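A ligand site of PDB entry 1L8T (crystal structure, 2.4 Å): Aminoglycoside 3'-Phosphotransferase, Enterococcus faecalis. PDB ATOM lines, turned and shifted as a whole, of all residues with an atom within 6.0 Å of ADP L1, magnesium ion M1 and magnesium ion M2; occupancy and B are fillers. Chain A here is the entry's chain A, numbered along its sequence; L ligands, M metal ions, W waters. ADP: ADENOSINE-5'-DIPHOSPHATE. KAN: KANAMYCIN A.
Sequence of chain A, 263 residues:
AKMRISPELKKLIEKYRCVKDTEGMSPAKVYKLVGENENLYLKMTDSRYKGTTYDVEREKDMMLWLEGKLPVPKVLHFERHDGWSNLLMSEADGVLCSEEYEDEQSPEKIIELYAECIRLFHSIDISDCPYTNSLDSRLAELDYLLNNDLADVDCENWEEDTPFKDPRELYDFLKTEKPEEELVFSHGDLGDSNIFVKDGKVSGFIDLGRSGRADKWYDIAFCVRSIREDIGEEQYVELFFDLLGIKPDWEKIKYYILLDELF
O7 of KAN L2 sits at hydrogen-bond distance from OD2 of Asp 189. The backbone NH (N) of Met 25 lies within hydrogen-bond range of an oxygen (O2B) of ADP L1, 3.5 Å away. The backbone carbonyl oxygen (O) of Ser 90 is in hydrogen-bond range of a nitrogen (N6) of ADP L1 (3.2 Å). The side-chain amino group of Lys 43 lies within salt-bridge range of an oxygen (O1A) of ADP L1, at 2.8 Å. OH of Tyr 41 sits close to N3 of ADP L1 (3.5 Å). O3' of ADP L1 lies within hydrogen-bond range of O of Ser 193 (2.8 Å). OE1 of Glu 23 is in hydrogen-bond range of O3' of ADP L1 (3.2 Å). An oxygen (O2B) of ADP L1 lies close to the backbone NH (N) of Ser 26. OG of Ser 26 lies within hydrogen-bond range of O2B of ADP L1 (2.6 Å). The backbone NH (N) of Ala 92 sits at hydrogen-bond distance from a nitrogen (N1) of ADP L1, 2.8 Å away. The side-chain hydroxyl (OG) of Ser 193 is in hydrogen-bond range of an oxygen (O3') of ADP L1 (3.2 Å).
The backbone NH (N) of Ala 28 sits close to the side-chain hydroxyl (OG) of Ser 26, at 3.1 Å. The side-chain carboxylate of Glu 59 sits close to the backbone NH of Asp 207. The backbone NH of Glu 23 is in hydrogen-bond range of the side-chain carboxylate of Asp 21, 3.0 Å away. N of Gly 24 sits at hydrogen-bond distance from OD2 of Asp 21 (2.7 Å). The backbone carbonyl oxygen (O) of Asn 194 lies within hydrogen-bond range of the backbone NH (N) of Ile 206, at 3.0 Å. The side-chain carboxylate of Asp 207 sits close to the side-chain amino group of Lys 43 (3.1 Å). The side-chain amide nitrogen (ND2) of Asn 194 lies within hydrogen-bond range of the backbone carbonyl oxygen (O) of Asp 189 (2.8 Å). O of Val 30 sits at hydrogen-bond distance from N of Asp 21.
The side-chain carboxylate (OD1) of Asp 21 lies close to an oxygen (O4') of ADP L1, 3.3 Å away. Merely in contact with ADP L1: Gly 24, Val 30, Pro 73, Met 89, Glu 91, Leu 96, Phe 196 and Ile 206. Hydrophobic or aromatic side chains within 4 Å of ADP L1: Val 30, Tyr 41, Pro 73, Met 89, Ala 92, Leu 96, Phe 196 and Ile 206. 19 residues have an atom within 4 Å of ADP L1: Asp 21, Glu 23, Gly 24, Met 25, Ser 26, Val 30, Tyr 41, Lys 43, Pro 73, Met 89, Ser 90, Glu 91, Ala 92, Leu 96, Ser 193, Asn 194, Phe 196, Ile 206 and Asp 207. The nearest printed residue that does not touch ADP L1 is Glu 59 (4.3 Å).
Ser 193 touches magnesium ion M1 (OG to MG, 3.97 Å). The nearest printed residue that does not touch magnesium ion M1 is Asp 189 (4.5 Å).
Residues that only touch magnesium ion M2: Ser 26 (3.9 Å). Of the 26 residues printed, 2 come within 4 Å of magnesium ion M2.
Magnesium ion M1 is bound by O2A of ADP L1 (1.8 Å), water W9 (1.8 Å), OD1 of Asn 194 (1.9 Å), OD2 of Asp 207 (2.0 Å), water W5 (2.0 Å) and O3B of ADP L1 (2.1 Å). Magnesium ion M1 has six donor atoms within binding distance.
Magnesium ion M2 is bound by water W2, an oxygen (O1B) of ADP L1, water W8, water W7, the side-chain carboxylate (OD1) of Asp 207 and the side-chain carboxylate (OD2) of Asp 207. Magnesium ion M2 has six donor atoms within binding distance.
Water W9 lies within hydrogen-bond range of an oxygen (O3') of ADP L1 (3.4 Å) and the backbone carbonyl oxygen (O) of Ser 193 (3.5 Å). Water W2 bridges OD2 of Asp 189 (2.5 Å) and O7 of KAN L2 (3.5 Å). Water W8 lies within hydrogen-bond range of an oxygen (O7) of KAN L2 (2.5 Å) and an oxygen (O2B) of ADP L1 (3.4 Å). Water W3 lies within hydrogen-bond range of an oxygen (O7) of KAN L2 and the backbone NH (N) of Met 25. Water W1 lies within hydrogen-bond range of an oxygen (O2B) of ADP L1, the backbone carbonyl oxygen of Ala 28, the backbone carbonyl oxygen of Gly 24 and the side-chain hydroxyl of Ser 26. Water W6 bridges N7 of ADP L1 (2.9 Å) and SD of Met 89 (3.5 Å).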
ATOM      1  N   ASP A  21      29.406 -13.941  13.655  1.00  0.00           N
ATOM      2  CA  ASP A  21      29.728 -13.364  12.355  1.00  0.00           C
ATOM      3  C   ASP A  21      31.239 -13.192  12.238  1.00  0.00           C
ATOM      4  O   ASP A  21      31.923 -13.032  13.247  1.00  0.00           O
ATOM      5  CB  ASP A  21      29.047 -12.000  12.184  1.00  0.00           C
ATOM      6  CG  ASP A  21      29.427 -11.308  10.874  1.00  0.00           C
ATOM      7  OD1 ASP A  21      28.984 -11.757   9.790  1.00  0.00           O
ATOM      8  OD2 ASP A  21      30.183 -10.300  10.929  1.00  0.00           O
ATOM      9  N   GLU A  23      32.340 -11.376   9.212  1.00  0.00           N
ATOM     10  CA  GLU A  23      32.451 -10.371   8.176  1.00  0.00           C
ATOM     11  C   GLU A  23      32.672  -8.973   8.761  1.00  0.00           C
ATOM     12  O   GLU A  23      33.581  -8.253   8.342  1.00  0.00           O
ATOM     13  CB  GLU A  23      31.202 -10.383   7.294  1.00  0.00           C
ATOM     14  CG  GLU A  23      31.165  -9.282   6.244  1.00  0.00           C
ATOM     15  CD  GLU A  23      30.375  -9.678   5.002  1.00  0.00           C
ATOM     16  OE1 GLU A  23      29.235 -10.165   5.154  1.00  0.00           O
ATOM     17  OE2 GLU A  23      30.903  -9.495   3.876  1.00  0.00           O
ATOM     18  N   GLY A  24      31.824  -8.595   9.706  1.00  0.00           N
ATOM     19  CA  GLY A  24      31.942  -7.297  10.340  1.00  0.00           C
ATOM     20  C   GLY A  24      33.362  -6.931  10.726  1.00  0.00           C
ATOM     21  O   GLY A  24      34.047  -7.685  11.433  1.00  0.00           O
ATOM     22  N   MET A  25      33.818  -5.772  10.273  1.00  0.00           N
ATOM     23  CA  MET A  25      35.158  -5.302  10.565  1.00  0.00           C
ATOM     24  C   MET A  25      35.144  -4.232  11.644  1.00  0.00           C
ATOM     25  O   MET A  25      36.193  -3.706  12.029  1.00  0.00           O
ATOM     26  CB  MET A  25      35.802  -4.739   9.297  1.00  0.00           C
ATOM     27  CG  MET A  25      36.124  -5.780   8.255  1.00  0.00           C
ATOM     28  SD  MET A  25      36.182  -5.074   6.602  1.00  0.00           S
ATOM     29  CE  MET A  25      37.713  -4.069   6.695  1.00  0.00           C
ATOM     30  N   SER A  26      33.963  -3.906  12.130  1.00  0.00           N
ATOM     31  CA  SER A  26      33.863  -2.883  13.159  1.00  0.00           C
ATOM     32  C   SER A  26      34.273  -3.461  14.503  1.00  0.00           C
ATOM     33  O   SER A  26      34.620  -4.637  14.606  1.00  0.00           O
ATOM     34  CB  SER A  26      32.417  -2.373  13.264  1.00  0.00           C
ATOM     35  OG  SER A  26      31.586  -3.324  13.878  1.00  0.00           O
ATOM     36  N   PRO A  27      34.290  -2.614  15.543  1.00  0.00           N
ATOM     37  CA  PRO A  27      34.670  -3.096  16.869  1.00  0.00           C
ATOM     38  C   PRO A  27      33.497  -3.875  17.488  1.00  0.00           C
ATOM     39  O   PRO A  27      33.630  -4.511  18.526  1.00  0.00           O
ATOM     40  CB  PRO A  27      34.957  -1.802  17.637  1.00  0.00           C
ATOM     41  CG  PRO A  27      35.265  -0.805  16.555  1.00  0.00           C
ATOM     42  CD  PRO A  27      34.264  -1.142  15.511  1.00  0.00           C
ATOM     43  N   ALA A  28      32.347  -3.824  16.837  1.00  0.00           N
ATOM     44  CA  ALA A  28      31.164  -4.509  17.341  1.00  0.00           C
ATOM     45  C   ALA A  28      31.228  -6.024  17.172  1.00  0.00           C
ATOM     46  O   ALA A  28      31.927  -6.528  16.273  1.00  0.00           O
ATOM     47  CB  ALA A  28      29.905  -3.949  16.658  1.00  0.00           C
ATOM     48  N   VAL A  30      29.097  -9.398  16.372  1.00  0.00           N
ATOM     49  CA  VAL A  30      27.861  -9.784  15.711  1.00  0.00           C
ATOM     50  C   VAL A  30      27.620 -11.274  15.756  1.00  0.00           C
ATOM     51  O   VAL A  30      28.501 -12.068  15.415  1.00  0.00           O
ATOM     52  CB  VAL A  30      27.889  -9.334  14.244  1.00  0.00           C
ATOM     53  CG1 VAL A  30      26.601  -9.729  13.547  1.00  0.00           C
ATOM     54  CG2 VAL A  30      28.098  -7.816  14.182  1.00  0.00           C
ATOM     55  N   TYR A  41      19.370 -11.616  15.254  1.00  0.00           N
ATOM     56  CA  TYR A  41      20.721 -11.105  15.246  1.00  0.00           C
ATOM     57  C   TYR A  41      21.025 -10.321  16.490  1.00  0.00           C
ATOM     58  O   TYR A  41      20.176  -9.562  16.987  1.00  0.00           O
ATOM     59  CB  TYR A  41      20.972 -10.245  14.018  1.00  0.00           C
ATOM     60  CG  TYR A  41      21.629 -11.026  12.904  1.00  0.00           C
ATOM     61  CD1 TYR A  41      20.859 -11.758  11.991  1.00  0.00           C
ATOM     62  CD2 TYR A  41      23.006 -11.083  12.795  1.00  0.00           C
ATOM     63  CE1 TYR A  41      21.466 -12.517  10.986  1.00  0.00           C
ATOM     64  CE2 TYR A  41      23.625 -11.841  11.811  1.00  0.00           C
ATOM     65  CZ  TYR A  41      22.849 -12.556  10.915  1.00  0.00           C
ATOM     66  OH  TYR A  41      23.483 -13.290   9.948  1.00  0.00           O
ATOM     67  N   LYS A  43      23.940  -7.801  18.165  1.00  0.00           N
ATOM     68  CA  LYS A  43      25.096  -6.949  17.903  1.00  0.00           C
ATOM     69  C   LYS A  43      25.391  -6.202  19.200  1.00  0.00           C
ATOM     70  O   LYS A  43      24.473  -5.761  19.895  1.00  0.00           O
ATOM     71  CB  LYS A  43      24.793  -5.946  16.786  1.00  0.00           C
ATOM     72  CG  LYS A  43      26.016  -5.207  16.274  1.00  0.00           C
ATOM     73  CD  LYS A  43      25.678  -4.278  15.112  1.00  0.00           C
ATOM     74  CE  LYS A  43      26.920  -3.722  14.455  1.00  0.00           C
ATOM     75  NZ  LYS A  43      26.608  -2.887  13.270  1.00  0.00           N
ATOM     76  N   TYR A  54      29.696   4.342  16.632  1.00  0.00           N
ATOM     77  CA  TYR A  54      29.864   2.898  16.657  1.00  0.00           C
ATOM     78  C   TYR A  54      28.904   2.275  17.666  1.00  0.00           C
ATOM     79  O   TYR A  54      28.505   1.114  17.537  1.00  0.00           O
ATOM     80  CB  TYR A  54      31.283   2.525  17.062  1.00  0.00           C
ATOM     81  CG  TYR A  54      32.366   2.878  16.078  1.00  0.00           C
ATOM     82  CD1 TYR A  54      33.230   3.949  16.307  1.00  0.00           C
ATOM     83  CD2 TYR A  54      32.545   2.127  14.918  1.00  0.00           C
ATOM     84  CE1 TYR A  54      34.254   4.253  15.404  1.00  0.00           C
ATOM     85  CE2 TYR A  54      33.558   2.420  14.022  1.00  0.00           C
ATOM     86  CZ  TYR A  54      34.411   3.480  14.259  1.00  0.00           C
ATOM     87  OH  TYR A  54      35.406   3.742  13.358  1.00  0.00           O
ATOM     88  N   GLU A  59      22.875   3.033  17.238  1.00  0.00           N
ATOM     89  CA  GLU A  59      22.427   2.223  16.109  1.00  0.00           C
ATOM     90  C   GLU A  59      20.987   1.797  16.346  1.00  0.00           C
ATOM     91  O   GLU A  59      20.181   1.757  15.410  1.00  0.00           O
ATOM     92  CB  GLU A  59      23.348   0.992  15.983  1.00  0.00           C
ATOM     93  CG  GLU A  59      22.977  -0.058  14.951  1.00  0.00           C
ATOM     94  CD  GLU A  59      24.171  -0.942  14.553  1.00  0.00           C
ATOM     95  OE1 GLU A  59      24.990  -1.300  15.426  1.00  0.00           O
ATOM     96  OE2 GLU A  59      24.285  -1.293  13.368  1.00  0.00           O
ATOM     97  N   PRO A  73      15.804  -3.650  10.395  1.00  0.00           N
ATOM     98  CA  PRO A  73      15.400  -4.744  11.270  1.00  0.00           C
ATOM     99  C   PRO A  73      14.447  -4.262  12.342  1.00  0.00           C
ATOM    100  O   PRO A  73      14.319  -3.061  12.587  1.00  0.00           O
ATOM    101  CB  PRO A  73      16.731  -5.236  11.851  1.00  0.00           C
ATOM    102  CG  PRO A  73      17.741  -4.835  10.792  1.00  0.00           C
ATOM    103  CD  PRO A  73      17.261  -3.464  10.425  1.00  0.00           C
ATOM    104  N   MET A  89      17.870  -8.023  17.284  1.00  0.00           N
ATOM    105  CA  MET A  89      17.031  -7.592  16.180  1.00  0.00           C
ATOM    106  C   MET A  89      16.630  -8.728  15.258  1.00  0.00           C
ATOM    107  O   MET A  89      17.194  -9.827  15.311  1.00  0.00           O
ATOM    108  CB  MET A  89      17.783  -6.554  15.353  1.00  0.00           C
ATOM    109  CG  MET A  89      18.941  -7.176  14.570  1.00  0.00           C
ATOM    110  SD  MET A  89      20.334  -6.085  14.334  1.00  0.00           S
ATOM    111  CE  MET A  89      20.375  -5.962  12.603  1.00  0.00           C
ATOM    112  N   SER A  90      15.654  -8.453  14.405  1.00  0.00           N
ATOM    113  CA  SER A  90      15.177  -9.451  13.461  1.00  0.00           C
ATOM    114  C   SER A  90      16.121  -9.527  12.264  1.00  0.00           C
ATOM    115  O   SER A  90      16.762  -8.552  11.909  1.00  0.00           O
ATOM    116  CB  SER A  90      13.777  -9.082  12.983  1.00  0.00           C
ATOM    117  OG  SER A  90      13.754  -7.789  12.410  1.00  0.00           O
ATOM    118  N   GLU A  91      16.197 -10.706  11.665  1.00  0.00           N
ATOM    119  CA  GLU A  91      17.044 -10.898  10.501  1.00  0.00           C
ATOM    120  C   GLU A  91      16.530 -10.038   9.355  1.00  0.00           C
ATOM    121  O   GLU A  91      15.327  -9.971   9.111  1.00  0.00           O
ATOM    122  CB  GLU A  91      17.050 -12.372  10.107  1.00  0.00           C
ATOM    123  CG  GLU A  91      17.719 -12.676   8.781  1.00  0.00           C
ATOM    124  CD  GLU A  91      17.832 -14.168   8.529  1.00  0.00           C
ATOM    125  OE1 GLU A  91      16.832 -14.876   8.806  1.00  0.00           O
ATOM    126  OE2 GLU A  91      18.906 -14.621   8.060  1.00  0.00           O
ATOM    127  N   ALA A  92      17.443  -9.373   8.652  1.00  0.00           N
ATOM    128  CA  ALA A  92      17.043  -8.536   7.530  1.00  0.00           C
ATOM    129  C   ALA A  92      16.420  -9.441   6.485  1.00  0.00           C
ATOM    130  O   ALA A  92      16.897 -10.544   6.228  1.00  0.00           O
ATOM    131  CB  ALA A  92      18.245  -7.824   6.946  1.00  0.00           C
ATOM    132  N   ASP A  93      15.330  -8.983   5.896  1.00  0.00           N
ATOM    133  CA  ASP A  93      14.680  -9.764   4.867  1.00  0.00           C
ATOM    134  C   ASP A  93      15.443  -9.580   3.557  1.00  0.00           C
ATOM    135  O   ASP A  93      15.931  -8.487   3.266  1.00  0.00           O
ATOM    136  CB  ASP A  93      13.232  -9.307   4.697  1.00  0.00           C
ATOM    137  CG  ASP A  93      12.546  -9.999   3.534  1.00  0.00           C
ATOM    138  OD1 ASP A  93      12.585 -11.258   3.476  1.00  0.00           O
ATOM    139  OD2 ASP A  93      11.966  -9.287   2.687  1.00  0.00           O
ATOM    140  N   LEU A  96      21.784 -10.629   1.257  1.00  0.00           N
ATOM    141  CA  LEU A  96      22.894  -9.711   1.384  1.00  0.00           C
ATOM    142  C   LEU A  96      23.362  -9.368  -0.033  1.00  0.00           C
ATOM    143  O   LEU A  96      23.686 -10.248  -0.812  1.00  0.00           O
ATOM    144  CB  LEU A  96      24.004 -10.407   2.167  1.00  0.00           C
ATOM    145  CG  LEU A  96      25.234  -9.725   2.732  1.00  0.00           C
ATOM    146  CD1 LEU A  96      24.864  -8.545   3.658  1.00  0.00           C
ATOM    147  CD2 LEU A  96      26.004 -10.796   3.484  1.00  0.00           C
ATOM    148  N   ASP A 189      27.458   4.173   6.088  1.00  0.00           N
ATOM    149  CA  ASP A 189      28.384   3.139   5.633  1.00  0.00           C
ATOM    150  C   ASP A 189      27.690   2.292   4.588  1.00  0.00           C
ATOM    151  O   ASP A 189      27.438   1.097   4.770  1.00  0.00           O
ATOM    152  CB  ASP A 189      28.854   2.294   6.820  1.00  0.00           C
ATOM    153  CG  ASP A 189      29.918   1.286   6.433  1.00  0.00           C
ATOM    154  OD1 ASP A 189      30.588   1.455   5.385  1.00  0.00           O
ATOM    155  OD2 ASP A 189      30.085   0.308   7.186  1.00  0.00           O
ATOM    156  N   SER A 193      27.744  -4.858   2.012  1.00  0.00           N
ATOM    157  CA  SER A 193      27.842  -5.649   3.235  1.00  0.00           C
ATOM    158  C   SER A 193      26.750  -5.239   4.237  1.00  0.00           C
ATOM    159  O   SER A 193      26.499  -5.942   5.205  1.00  0.00           O
ATOM    160  CB  SER A 193      29.221  -5.438   3.838  1.00  0.00           C
ATOM    161  OG  SER A 193      29.351  -6.069   5.097  1.00  0.00           O
ATOM    162  N   ASN A 194      26.105  -4.105   3.982  1.00  0.00           N
ATOM    163  CA  ASN A 194      25.068  -3.597   4.864  1.00  0.00           C
ATOM    164  C   ASN A 194      23.715  -3.418   4.177  1.00  0.00           C
ATOM    165  O   ASN A 194      22.770  -2.909   4.788  1.00  0.00           O
ATOM    166  CB  ASN A 194      25.513  -2.258   5.471  1.00  0.00           C
ATOM    167  CG  ASN A 194      26.859  -2.343   6.169  1.00  0.00           C
ATOM    168  OD1 ASN A 194      27.093  -3.243   6.977  1.00  0.00           O
ATOM    169  ND2 ASN A 194      27.753  -1.417   5.868  1.00  0.00           N
ATOM    170  N   PHE A 196      20.527  -5.239   1.776  1.00  0.00           N
ATOM    171  CA  PHE A 196      19.867  -6.496   1.372  1.00  0.00           C
ATOM    172  C   PHE A 196      18.981  -6.285   0.160  1.00  0.00           C
ATOM    173  O   PHE A 196      18.343  -5.250   0.008  1.00  0.00           O
ATOM    174  CB  PHE A 196      19.043  -7.051   2.523  1.00  0.00           C
ATOM    175  CG  PHE A 196      19.879  -7.520   3.671  1.00  0.00           C
ATOM    176  CD1 PHE A 196      20.480  -6.605   4.523  1.00  0.00           C
ATOM    177  CD2 PHE A 196      20.118  -8.886   3.854  1.00  0.00           C
ATOM    178  CE1 PHE A 196      21.321  -7.040   5.542  1.00  0.00           C
ATOM    179  CE2 PHE A 196      20.958  -9.321   4.872  1.00  0.00           C
ATOM    180  CZ  PHE A 196      21.570  -8.394   5.717  1.00  0.00           C
ATOM    181  N   ILE A 206      21.179  -2.399   7.259  1.00  0.00           N
ATOM    182  CA  ILE A 206      21.663  -2.679   8.613  1.00  0.00           C
ATOM    183  C   ILE A 206      22.878  -1.786   8.870  1.00  0.00           C
ATOM    184  O   ILE A 206      23.236  -0.979   8.016  1.00  0.00           O
ATOM    185  CB  ILE A 206      22.107  -4.171   8.782  1.00  0.00           C
ATOM    186  CG1 ILE A 206      23.136  -4.538   7.713  1.00  0.00           C
ATOM    187  CG2 ILE A 206      20.899  -5.083   8.684  1.00  0.00           C
ATOM    188  CD1 ILE A 206      23.874  -5.830   7.982  1.00  0.00           C
ATOM    189  N   ASP A 207      23.512  -1.933  10.038  1.00  0.00           N
ATOM    190  CA  ASP A 207      24.690  -1.159  10.383  1.00  0.00           C
ATOM    191  C   ASP A 207      24.260   0.313  10.341  1.00  0.00           C
ATOM    192  O   ASP A 207      24.567   1.015   9.387  1.00  0.00           O
ATOM    193  CB  ASP A 207      25.780  -1.421   9.333  1.00  0.00           C
ATOM    194  CG  ASP A 207      27.175  -1.514   9.930  1.00  0.00           C
ATOM    195  OD1 ASP A 207      27.438  -0.909  11.000  1.00  0.00           O
ATOM    196  OD2 ASP A 207      28.018  -2.171   9.306  1.00  0.00           O
ATOM    197  N   ARG A 210      25.930   4.904  12.342  1.00  0.00           N
ATOM    198  CA  ARG A 210      26.433   6.122  11.709  1.00  0.00           C
ATOM    199  C   ARG A 210      25.375   6.868  10.901  1.00  0.00           C
ATOM    200  O   ARG A 210      25.707   7.822  10.195  1.00  0.00           O
ATOM    201  CB  ARG A 210      27.598   5.762  10.796  1.00  0.00           C
ATOM    202  CG  ARG A 210      28.633   6.847  10.632  1.00  0.00           C
ATOM    203  CD  ARG A 210      29.800   6.354   9.777  1.00  0.00           C
ATOM    204  NE  ARG A 210      30.493   5.186  10.335  1.00  0.00           N
ATOM    205  CZ  ARG A 210      31.084   5.153  11.533  1.00  0.00           C
ATOM    206  NH1 ARG A 210      31.058   6.220  12.305  1.00  0.00           N
ATOM    207  NH2 ARG A 210      31.692   4.063  11.964  1.00  0.00           N
HETATM  208  PB  ADP L   1      29.659  -4.087  11.281  1.00  0.00           P
HETATM  209  O1B ADP L   1      29.265  -2.761  11.757  1.00  0.00           O
HETATM  210  O2B ADP L   1      30.851  -4.749  11.802  1.00  0.00           O
HETATM  211  O3B ADP L   1      29.832  -4.031   9.695  1.00  0.00           O
HETATM  212  PA  ADP L   1      27.139  -5.292  10.632  1.00  0.00           P
HETATM  213  O1A ADP L   1      25.944  -4.766  11.348  1.00  0.00           O
HETATM  214  O2A ADP L   1      27.451  -4.837   9.265  1.00  0.00           O
HETATM  215  O3A ADP L   1      28.421  -5.067  11.563  1.00  0.00           O
HETATM  216  O5' ADP L   1      27.022  -6.880  10.601  1.00  0.00           O
HETATM  217  C5' ADP L   1      28.077  -7.670  10.045  1.00  0.00           C
HETATM  218  C4' ADP L   1      27.493  -8.718   9.112  1.00  0.00           C
HETATM  219  O4' ADP L   1      26.558  -9.534   9.820  1.00  0.00           O
HETATM  220  C3' ADP L   1      26.643  -8.128   7.963  1.00  0.00           C
HETATM  221  O3' ADP L   1      27.457  -7.995   6.789  1.00  0.00           O
HETATM  222  C2' ADP L   1      25.623  -9.246   7.759  1.00  0.00           C
HETATM  223  O2' ADP L   1      26.239 -10.311   7.030  1.00  0.00           O
HETATM  224  C1' ADP L   1      25.319  -9.758   9.144  1.00  0.00           C
HETATM  225  N9  ADP L   1      24.129  -9.162   9.785  1.00  0.00           N
HETATM  226  C8  ADP L   1      24.049  -8.246  10.816  1.00  0.00           C
HETATM  227  N7  ADP L   1      22.826  -7.927  11.160  1.00  0.00           N
HETATM  228  C5  ADP L   1      22.052  -8.682  10.299  1.00  0.00           C
HETATM  229  C6  ADP L   1      20.637  -8.817  10.126  1.00  0.00           C
HETATM  230  N6  ADP L   1      19.746  -8.168  10.867  1.00  0.00           N
HETATM  231  N1  ADP L   1      20.203  -9.678   9.156  1.00  0.00           N
HETATM  232  C2  ADP L   1      21.094 -10.348   8.394  1.00  0.00           C
HETATM  233  N3  ADP L   1      22.425 -10.305   8.467  1.00  0.00           N
HETATM  234  C4  ADP L   1      22.840  -9.430   9.457  1.00  0.00           C
HETATM  235  C1  KAN L   2      35.677  -1.012   6.760  1.00  0.00           C
HETATM  236  C2  KAN L   2      34.241  -1.520   6.782  1.00  0.00           C
HETATM  237  C3  KAN L   2      33.430  -0.742   7.788  1.00  0.00           C
HETATM  238  C4  KAN L   2      34.096  -0.843   9.142  1.00  0.00           C
HETATM  239  C5  KAN L   2      35.479  -0.241   9.036  1.00  0.00           C
HETATM  240  C6  KAN L   2      36.185  -0.319  10.389  1.00  0.00           C
HETATM  241  C7  KAN L   2      38.305   2.095   3.498  1.00  0.00           C
HETATM  242  C8  KAN L   2      37.906   0.628   3.264  1.00  0.00           C
HETATM  243  C9  KAN L   2      36.663   0.284   4.121  1.00  0.00           C
HETATM  244  C10 KAN L   2      36.899   0.596   5.600  1.00  0.00           C
HETATM  245  C11 KAN L   2      37.240   2.083   5.738  1.00  0.00           C
HETATM  246  C12 KAN L   2      38.526   2.383   4.984  1.00  0.00           C
HETATM  247  C13 KAN L   2      37.943  -0.808   1.413  1.00  0.00           C
HETATM  248  C14 KAN L   2      38.637  -0.739   0.044  1.00  0.00           C
HETATM  249  C15 KAN L   2      37.693  -0.208  -1.020  1.00  0.00           C
HETATM  250  C16 KAN L   2      36.413  -0.998  -1.023  1.00  0.00           C
HETATM  251  C17 KAN L   2      35.791  -0.898   0.371  1.00  0.00           C
HETATM  252  C18 KAN L   2      34.474  -1.653   0.421  1.00  0.00           C
HETATM  253  N1  KAN L   2      37.491   0.342  10.315  1.00  0.00           N
HETATM  254  N2  KAN L   2      37.427   2.425   7.163  1.00  0.00           N
HETATM  255  N3  KAN L   2      39.542   2.398   2.759  1.00  0.00           N
HETATM  256  N4  KAN L   2      38.346  -0.317  -2.328  1.00  0.00           N
HETATM  257  O5  KAN L   2      36.260  -0.980   8.088  1.00  0.00           O
HETATM  258  O6  KAN L   2      33.657  -1.333   5.491  1.00  0.00           O
HETATM  259  O7  KAN L   2      32.145  -1.320   7.858  1.00  0.00           O
HETATM  260  O8  KAN L   2      33.330  -0.085  10.072  1.00  0.00           O
HETATM  261  O9  KAN L   2      35.712   0.357   6.347  1.00  0.00           O
HETATM  262  O10 KAN L   2      36.373  -1.102   3.996  1.00  0.00           O
HETATM  263  O11 KAN L   2      37.575   0.492   1.890  1.00  0.00           O
HETATM  264  O12 KAN L   2      36.684  -1.503   1.329  1.00  0.00           O
HETATM  265  O13 KAN L   2      39.733   0.141   0.145  1.00  0.00           O
HETATM  266  O14 KAN L   2      35.544  -0.395  -1.975  1.00  0.00           O
HETATM  267  O15 KAN L   2      33.598  -0.925   1.280  1.00  0.00           O
HETATM  268 MG    MG M   1      28.416  -3.748   8.179  1.00  0.00          MG
HETATM  269 MG    MG M   2      29.600  -0.999  10.981  1.00  0.00          MG
HETATM  270  O   HOH W   1      32.180  -6.568  13.383  1.00  0.00           O
HETATM  271  O   HOH W   2      29.569   0.253   9.625  1.00  0.00           O
HETATM  272  O   HOH W   3      32.382  -3.701   8.745  1.00  0.00           O
HETATM  273  O   HOH W   4      24.242 -11.762   6.110  1.00  0.00           O
HETATM  274  O   HOH W   5      30.002  -2.631   7.587  1.00  0.00           O
HETATM  275  O   HOH W   6      23.254  -5.435  12.576  1.00  0.00           O
HETATM  276  O   HOH W   7      30.387   0.406  12.151  1.00  0.00           O
HETATM  277  O   HOH W   8      31.134  -1.839  10.090  1.00  0.00           O
HETATM  278  O   HOH W   9      29.204  -5.098   7.226  1.00  0.00           O
